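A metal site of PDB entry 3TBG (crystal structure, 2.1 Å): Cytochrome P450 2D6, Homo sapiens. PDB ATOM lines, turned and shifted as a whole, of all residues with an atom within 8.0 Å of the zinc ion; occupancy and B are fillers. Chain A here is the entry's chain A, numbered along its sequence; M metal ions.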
ATOM      1  N   TRP A 130       5.780   4.743   7.013  1.00  0.00           N
ATOM      2  CA  TRP A 130       6.714   4.584   8.134  1.00  0.00           C
ATOM      3  C   TRP A 130       6.347   5.550   9.269  1.00  0.00           C
ATOM      4  O   TRP A 130       6.388   5.172  10.450  1.00  0.00           O
ATOM      5  CB  TRP A 130       8.152   4.857   7.685  1.00  0.00           C
ATOM      6  CG  TRP A 130       8.758   3.805   6.799  1.00  0.00           C
ATOM      7  CD1 TRP A 130       8.686   2.446   6.963  1.00  0.00           C
ATOM      8  CD2 TRP A 130       9.582   4.031   5.645  1.00  0.00           C
ATOM      9  NE1 TRP A 130       9.427   1.815   5.991  1.00  0.00           N
ATOM     10  CE2 TRP A 130       9.977   2.760   5.164  1.00  0.00           C
ATOM     11  CE3 TRP A 130      10.018   5.181   4.980  1.00  0.00           C
ATOM     12  CZ2 TRP A 130      10.803   2.619   4.039  1.00  0.00           C
ATOM     13  CZ3 TRP A 130      10.844   5.039   3.855  1.00  0.00           C
ATOM     14  CH2 TRP A 130      11.230   3.755   3.401  1.00  0.00           C
ATOM     15  N   ALA A 165      15.627   6.677  10.509  1.00  0.00           N
ATOM     16  CA  ALA A 165      16.142   5.331  10.345  1.00  0.00           C
ATOM     17  C   ALA A 165      15.399   4.646   9.210  1.00  0.00           C
ATOM     18  O   ALA A 165      16.002   3.923   8.416  1.00  0.00           O
ATOM     19  CB  ALA A 165      15.972   4.533  11.644  1.00  0.00           C
ATOM     20  N   SER A 166      14.083   4.857   9.138  1.00  0.00           N
ATOM     21  CA  SER A 166      13.272   4.253   8.073  1.00  0.00           C
ATOM     22  C   SER A 166      13.677   4.821   6.717  1.00  0.00           C
ATOM     23  O   SER A 166      13.831   4.087   5.752  1.00  0.00           O
ATOM     24  CB  SER A 166      11.779   4.517   8.310  1.00  0.00           C
ATOM     25  OG  SER A 166      11.366   3.974   9.542  1.00  0.00           O
ATOM     26  N   LEU A 167      13.838   6.141   6.661  1.00  0.00           N
ATOM     27  CA  LEU A 167      14.236   6.848   5.440  1.00  0.00           C
ATOM     28  C   LEU A 167      15.598   6.434   4.920  1.00  0.00           C
ATOM     29  O   LEU A 167      15.778   6.209   3.728  1.00  0.00           O
ATOM     30  CB  LEU A 167      14.253   8.363   5.687  1.00  0.00           C
ATOM     31  CG  LEU A 167      15.186   9.191   4.777  1.00  0.00           C
ATOM     32  CD1 LEU A 167      14.624   9.246   3.366  1.00  0.00           C
ATOM     33  CD2 LEU A 167      15.337  10.616   5.331  1.00  0.00           C
ATOM     34  N   THR A 168      16.574   6.345   5.836  1.00  0.00           N
ATOM     35  CA  THR A 168      17.943   6.014   5.473  1.00  0.00           C
ATOM     36  C   THR A 168      18.287   4.531   5.402  1.00  0.00           C
ATOM     37  O   THR A 168      18.968   4.114   4.475  1.00  0.00           O
ATOM     38  CB  THR A 168      18.932   6.664   6.457  1.00  0.00           C
ATOM     39  OG1 THR A 168      18.667   6.186   7.778  1.00  0.00           O
ATOM     40  CG2 THR A 168      18.818   8.177   6.422  1.00  0.00           C
ATOM     41  N   CYS A 169      17.833   3.738   6.372  1.00  0.00           N
ATOM     42  CA  CYS A 169      18.154   2.309   6.419  1.00  0.00           C
ATOM     43  C   CYS A 169      16.989   1.366   6.156  1.00  0.00           C
ATOM     44  O   CYS A 169      17.169   0.154   6.122  1.00  0.00           O
ATOM     45  CB  CYS A 169      18.757   1.954   7.781  1.00  0.00           C
ATOM     46  SG  CYS A 169      20.080   3.033   8.337  1.00  0.00           S
ATOM     47  N   GLY A 170      15.794   1.911   5.980  1.00  0.00           N
ATOM     48  CA  GLY A 170      14.646   1.061   5.728  1.00  0.00           C
ATOM     49  C   GLY A 170      14.220   0.197   6.913  1.00  0.00           C
ATOM     50  O   GLY A 170      13.690  -0.903   6.722  1.00  0.00           O
ATOM     51  N   ARG A 171      14.442   0.661   8.137  1.00  0.00           N
ATOM     52  CA  ARG A 171      14.057  -0.110   9.327  1.00  0.00           C
ATOM     53  C   ARG A 171      13.855   0.815  10.508  1.00  0.00           C
ATOM     54  O   ARG A 171      14.234   1.985  10.469  1.00  0.00           O
ATOM     55  CB  ARG A 171      15.153  -1.087   9.723  1.00  0.00           C
ATOM     56  CG  ARG A 171      16.399  -0.390  10.265  1.00  0.00           C
ATOM     57  CD  ARG A 171      17.279  -1.352  11.049  1.00  0.00           C
ATOM     58  NE  ARG A 171      16.591  -1.818  12.246  1.00  0.00           N
ATOM     59  CZ  ARG A 171      17.075  -2.719  13.094  1.00  0.00           C
ATOM     60  NH1 ARG A 171      18.258  -3.286  12.867  1.00  0.00           N
ATOM     61  NH2 ARG A 171      16.359  -3.054  14.163  1.00  0.00           N
ATOM     62  N   HIS A 236      23.280  -3.075   6.903  1.00  0.00           N
ATOM     63  CA  HIS A 236      22.334  -2.766   5.840  1.00  0.00           C
ATOM     64  C   HIS A 236      22.892  -3.182   4.492  1.00  0.00           C
ATOM     65  O   HIS A 236      22.164  -3.652   3.634  1.00  0.00           O
ATOM     66  CB  HIS A 236      22.044  -1.258   5.794  1.00  0.00           C
ATOM     67  CG  HIS A 236      20.926  -0.894   4.854  1.00  0.00           C
ATOM     68  ND1 HIS A 236      20.630   0.413   4.534  1.00  0.00           N
ATOM     69  CD2 HIS A 236      20.034  -1.654   4.187  1.00  0.00           C
ATOM     70  CE1 HIS A 236      19.598   0.441   3.713  1.00  0.00           C
ATOM     71  NE2 HIS A 236      19.221  -0.795   3.484  1.00  0.00           N
ATOM     72  N   ARG A 237      24.191  -2.983   4.311  1.00  0.00           N
ATOM     73  CA  ARG A 237      24.880  -3.312   3.067  1.00  0.00           C
ATOM     74  C   ARG A 237      24.740  -4.798   2.805  1.00  0.00           C
ATOM     75  O   ARG A 237      24.649  -5.232   1.658  1.00  0.00           O
ATOM     76  CB  ARG A 237      26.359  -2.913   3.178  1.00  0.00           C
ATOM     77  CG  ARG A 237      27.226  -3.270   1.970  1.00  0.00           C
ATOM     78  CD  ARG A 237      27.815  -2.038   1.267  1.00  0.00           C
ATOM     79  NE  ARG A 237      28.394  -1.069   2.204  1.00  0.00           N
ATOM     80  CZ  ARG A 237      29.167  -0.038   1.847  1.00  0.00           C
ATOM     81  NH1 ARG A 237      29.472   0.158   0.566  1.00  0.00           N
ATOM     82  NH2 ARG A 237      29.627   0.803   2.760  1.00  0.00           N
ATOM     83  N   THR A 239      22.151  -6.660   3.811  1.00  0.00           N
ATOM     84  CA  THR A 239      20.770  -7.015   3.516  1.00  0.00           C
ATOM     85  C   THR A 239      20.192  -6.404   2.230  1.00  0.00           C
ATOM     86  O   THR A 239      19.140  -6.817   1.763  1.00  0.00           O
ATOM     87  CB  THR A 239      19.837  -6.659   4.700  1.00  0.00           C
ATOM     88  OG1 THR A 239      19.857  -5.250   4.943  1.00  0.00           O
ATOM     89  CG2 THR A 239      20.297  -7.384   5.962  1.00  0.00           C
ATOM     90  N   TRP A 240      20.905  -5.437   1.657  1.00  0.00           N
ATOM     91  CA  TRP A 240      20.460  -4.774   0.440  1.00  0.00           C
ATOM     92  C   TRP A 240      20.308  -5.739  -0.733  1.00  0.00           C
ATOM     93  O   TRP A 240      21.186  -6.553  -0.995  1.00  0.00           O
ATOM     94  CB  TRP A 240      21.479  -3.690   0.050  1.00  0.00           C
ATOM     95  CG  TRP A 240      21.255  -3.068  -1.304  1.00  0.00           C
ATOM     96  CD1 TRP A 240      20.060  -2.698  -1.858  1.00  0.00           C
ATOM     97  CD2 TRP A 240      22.268  -2.631  -2.223  1.00  0.00           C
ATOM     98  NE1 TRP A 240      20.268  -2.060  -3.055  1.00  0.00           N
ATOM     99  CE2 TRP A 240      21.612  -1.998  -3.298  1.00  0.00           C
ATOM    100  CE3 TRP A 240      23.668  -2.710  -2.237  1.00  0.00           C
ATOM    101  CZ2 TRP A 240      22.314  -1.444  -4.387  1.00  0.00           C
ATOM    102  CZ3 TRP A 240      24.367  -2.163  -3.320  1.00  0.00           C
ATOM    103  CH2 TRP A 240      23.683  -1.544  -4.374  1.00  0.00           C
ATOM    104  N   ASP A 241      19.175  -5.643  -1.421  1.00  0.00           N
ATOM    105  CA  ASP A 241      18.915  -6.466  -2.593  1.00  0.00           C
ATOM    106  C   ASP A 241      18.979  -5.530  -3.808  1.00  0.00           C
ATOM    107  O   ASP A 241      17.995  -4.899  -4.158  1.00  0.00           O
ATOM    108  CB  ASP A 241      17.527  -7.113  -2.511  1.00  0.00           C
ATOM    109  CG  ASP A 241      17.254  -8.056  -3.676  1.00  0.00           C
ATOM    110  OD1 ASP A 241      16.206  -8.736  -3.680  1.00  0.00           O
ATOM    111  OD2 ASP A 241      18.088  -8.105  -4.590  1.00  0.00           O
ATOM    112  N   PRO A 245      14.237  -2.355  -6.800  1.00  0.00           N
ATOM    113  CA  PRO A 245      14.419  -0.897  -6.770  1.00  0.00           C
ATOM    114  C   PRO A 245      14.804  -0.484  -5.349  1.00  0.00           C
ATOM    115  O   PRO A 245      14.402  -1.136  -4.381  1.00  0.00           O
ATOM    116  CB  PRO A 245      13.045  -0.364  -7.154  1.00  0.00           C
ATOM    117  CG  PRO A 245      12.510  -1.453  -8.063  1.00  0.00           C
ATOM    118  CD  PRO A 245      12.906  -2.704  -7.317  1.00  0.00           C
ATOM    119  N   PRO A 246      15.596   0.591  -5.204  1.00  0.00           N
ATOM    120  CA  PRO A 246      16.006   1.072  -3.883  1.00  0.00           C
ATOM    121  C   PRO A 246      14.801   1.237  -2.972  1.00  0.00           C
ATOM    122  O   PRO A 246      13.801   1.831  -3.365  1.00  0.00           O
ATOM    123  CB  PRO A 246      16.678   2.394  -4.204  1.00  0.00           C
ATOM    124  CG  PRO A 246      17.300   2.141  -5.527  1.00  0.00           C
ATOM    125  CD  PRO A 246      16.202   1.394  -6.270  1.00  0.00           C
ATOM    126  N   ARG A 247      14.883   0.718  -1.757  1.00  0.00           N
ATOM    127  CA  ARG A 247      13.783   0.791  -0.812  1.00  0.00           C
ATOM    128  C   ARG A 247      13.933   1.976   0.157  1.00  0.00           C
ATOM    129  O   ARG A 247      12.975   2.392   0.795  1.00  0.00           O
ATOM    130  CB  ARG A 247      13.752  -0.505  -0.002  1.00  0.00           C
ATOM    131  CG  ARG A 247      12.379  -0.995   0.329  1.00  0.00           C
ATOM    132  CD  ARG A 247      12.482  -2.316   1.061  1.00  0.00           C
ATOM    133  NE  ARG A 247      13.197  -2.137   2.309  1.00  0.00           N
ATOM    134  CZ  ARG A 247      12.647  -1.686   3.433  1.00  0.00           C
ATOM    135  NH1 ARG A 247      11.354  -1.387   3.471  1.00  0.00           N
ATOM    136  NH2 ARG A 247      13.394  -1.520   4.505  1.00  0.00           N
ATOM    137  N   ASP A 248      15.154   2.488   0.245  1.00  0.00           N
ATOM    138  CA  ASP A 248      15.446   3.599   1.148  1.00  0.00           C
ATOM    139  C   ASP A 248      16.607   4.408   0.578  1.00  0.00           C
ATOM    140  O   ASP A 248      17.199   4.031  -0.428  1.00  0.00           O
ATOM    141  CB  ASP A 248      15.789   3.049   2.527  1.00  0.00           C
ATOM    142  CG  ASP A 248      16.759   1.880   2.455  1.00  0.00           C
ATOM    143  OD1 ASP A 248      17.856   2.060   1.892  1.00  0.00           O
ATOM    144  OD2 ASP A 248      16.425   0.788   2.952  1.00  0.00           O
ATOM    145  N   LEU A 249      16.932   5.518   1.244  1.00  0.00           N
ATOM    146  CA  LEU A 249      17.971   6.409   0.770  1.00  0.00           C
ATOM    147  C   LEU A 249      19.366   5.811   0.690  1.00  0.00           C
ATOM    148  O   LEU A 249      20.119   6.108  -0.244  1.00  0.00           O
ATOM    149  CB  LEU A 249      17.982   7.704   1.624  1.00  0.00           C
ATOM    150  CG  LEU A 249      18.917   8.813   1.112  1.00  0.00           C
ATOM    151  CD1 LEU A 249      18.404  10.181   1.532  1.00  0.00           C
ATOM    152  CD2 LEU A 249      20.313   8.575   1.637  1.00  0.00           C
ATOM    153  N   THR A 250      19.730   4.949   1.636  1.00  0.00           N
ATOM    154  CA  THR A 250      21.056   4.331   1.599  1.00  0.00           C
ATOM    155  C   THR A 250      21.171   3.385   0.394  1.00  0.00           C
ATOM    156  O   THR A 250      22.237   3.287  -0.223  1.00  0.00           O
ATOM    157  CB  THR A 250      21.358   3.574   2.918  1.00  0.00           C
ATOM    158  OG1 THR A 250      21.461   4.515   3.991  1.00  0.00           O
ATOM    159  CG2 THR A 250      22.670   2.812   2.805  1.00  0.00           C
ATOM    160  N   GLU A 251      20.088   2.707   0.046  1.00  0.00           N
ATOM    161  CA  GLU A 251      20.139   1.784  -1.100  1.00  0.00           C
ATOM    162  C   GLU A 251      20.274   2.604  -2.390  1.00  0.00           C
ATOM    163  O   GLU A 251      20.982   2.201  -3.307  1.00  0.00           O
ATOM    164  CB  GLU A 251      18.892   0.892  -1.138  1.00  0.00           C
ATOM    165  CG  GLU A 251      18.935  -0.184  -0.068  1.00  0.00           C
ATOM    166  CD  GLU A 251      17.695  -1.067  -0.036  1.00  0.00           C
ATOM    167  OE1 GLU A 251      16.978  -1.139  -1.048  1.00  0.00           O
ATOM    168  OE2 GLU A 251      17.467  -1.717   1.010  1.00  0.00           O
ATOM    169  N   ALA A 252      19.609   3.744  -2.454  1.00  0.00           N
ATOM    170  CA  ALA A 252      19.702   4.589  -3.632  1.00  0.00           C
ATOM    171  C   ALA A 252      21.137   5.107  -3.753  1.00  0.00           C
ATOM    172  O   ALA A 252      21.681   5.181  -4.838  1.00  0.00           O
ATOM    173  CB  ALA A 252      18.713   5.744  -3.537  1.00  0.00           C
ATOM    174  N   LEU A 254      23.899   3.647  -2.514  1.00  0.00           N
ATOM    175  CA  LEU A 254      24.742   2.505  -2.852  1.00  0.00           C
ATOM    176  C   LEU A 254      24.672   2.194  -4.350  1.00  0.00           C
ATOM    177  O   LEU A 254      25.690   1.955  -4.979  1.00  0.00           O
ATOM    178  CB  LEU A 254      24.327   1.261  -2.040  1.00  0.00           C
ATOM    179  CG  LEU A 254      24.574   1.332  -0.530  1.00  0.00           C
ATOM    180  CD1 LEU A 254      24.019   0.070   0.141  1.00  0.00           C
ATOM    181  CD2 LEU A 254      26.060   1.452  -0.256  1.00  0.00           C
HETATM  182 ZN    ZN M   1      17.393  -0.979   2.749  1.00  0.00          ZN
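The zinc ion is bound by OE2 of Glu 251, NE2 of His 236 and OD2 of Asp 248. The zinc ion has three donor atoms within binding distance.
Residues that only touch the zinc ion: Cys 169. Four residues have an atom within 4 Å of the zinc ion: Cys 169, His 236, Asp 248 and Glu 251.
The side-chain carboxylate (OE1) of Glu 251 lies within hydrogen-bond range of the backbone NH (N) of Arg 247 (2.9 Å). A ring nitrogen (NE2) of His 236 lies close to the backbone carbonyl oxygen (O) of Cys 169 (3.5 Å). The side-chain hydroxyl (OG1) of Thr 239 lies within hydrogen-bond range of the backbone carbonyl oxygen (O) of His 236, at 3.1 Å. OD2 of Asp 248 sits close to N of Gly 170, at 3.3 Å. The backbone NH of Thr 250 lies close to the side-chain carboxylate of Asp 248 (3.5 Å). The side-chain hydroxyl (OG1) of Thr 168 lies within hydrogen-bond range of the side-chain sulfur (SG) of Cys 169, 3.5 Å away.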
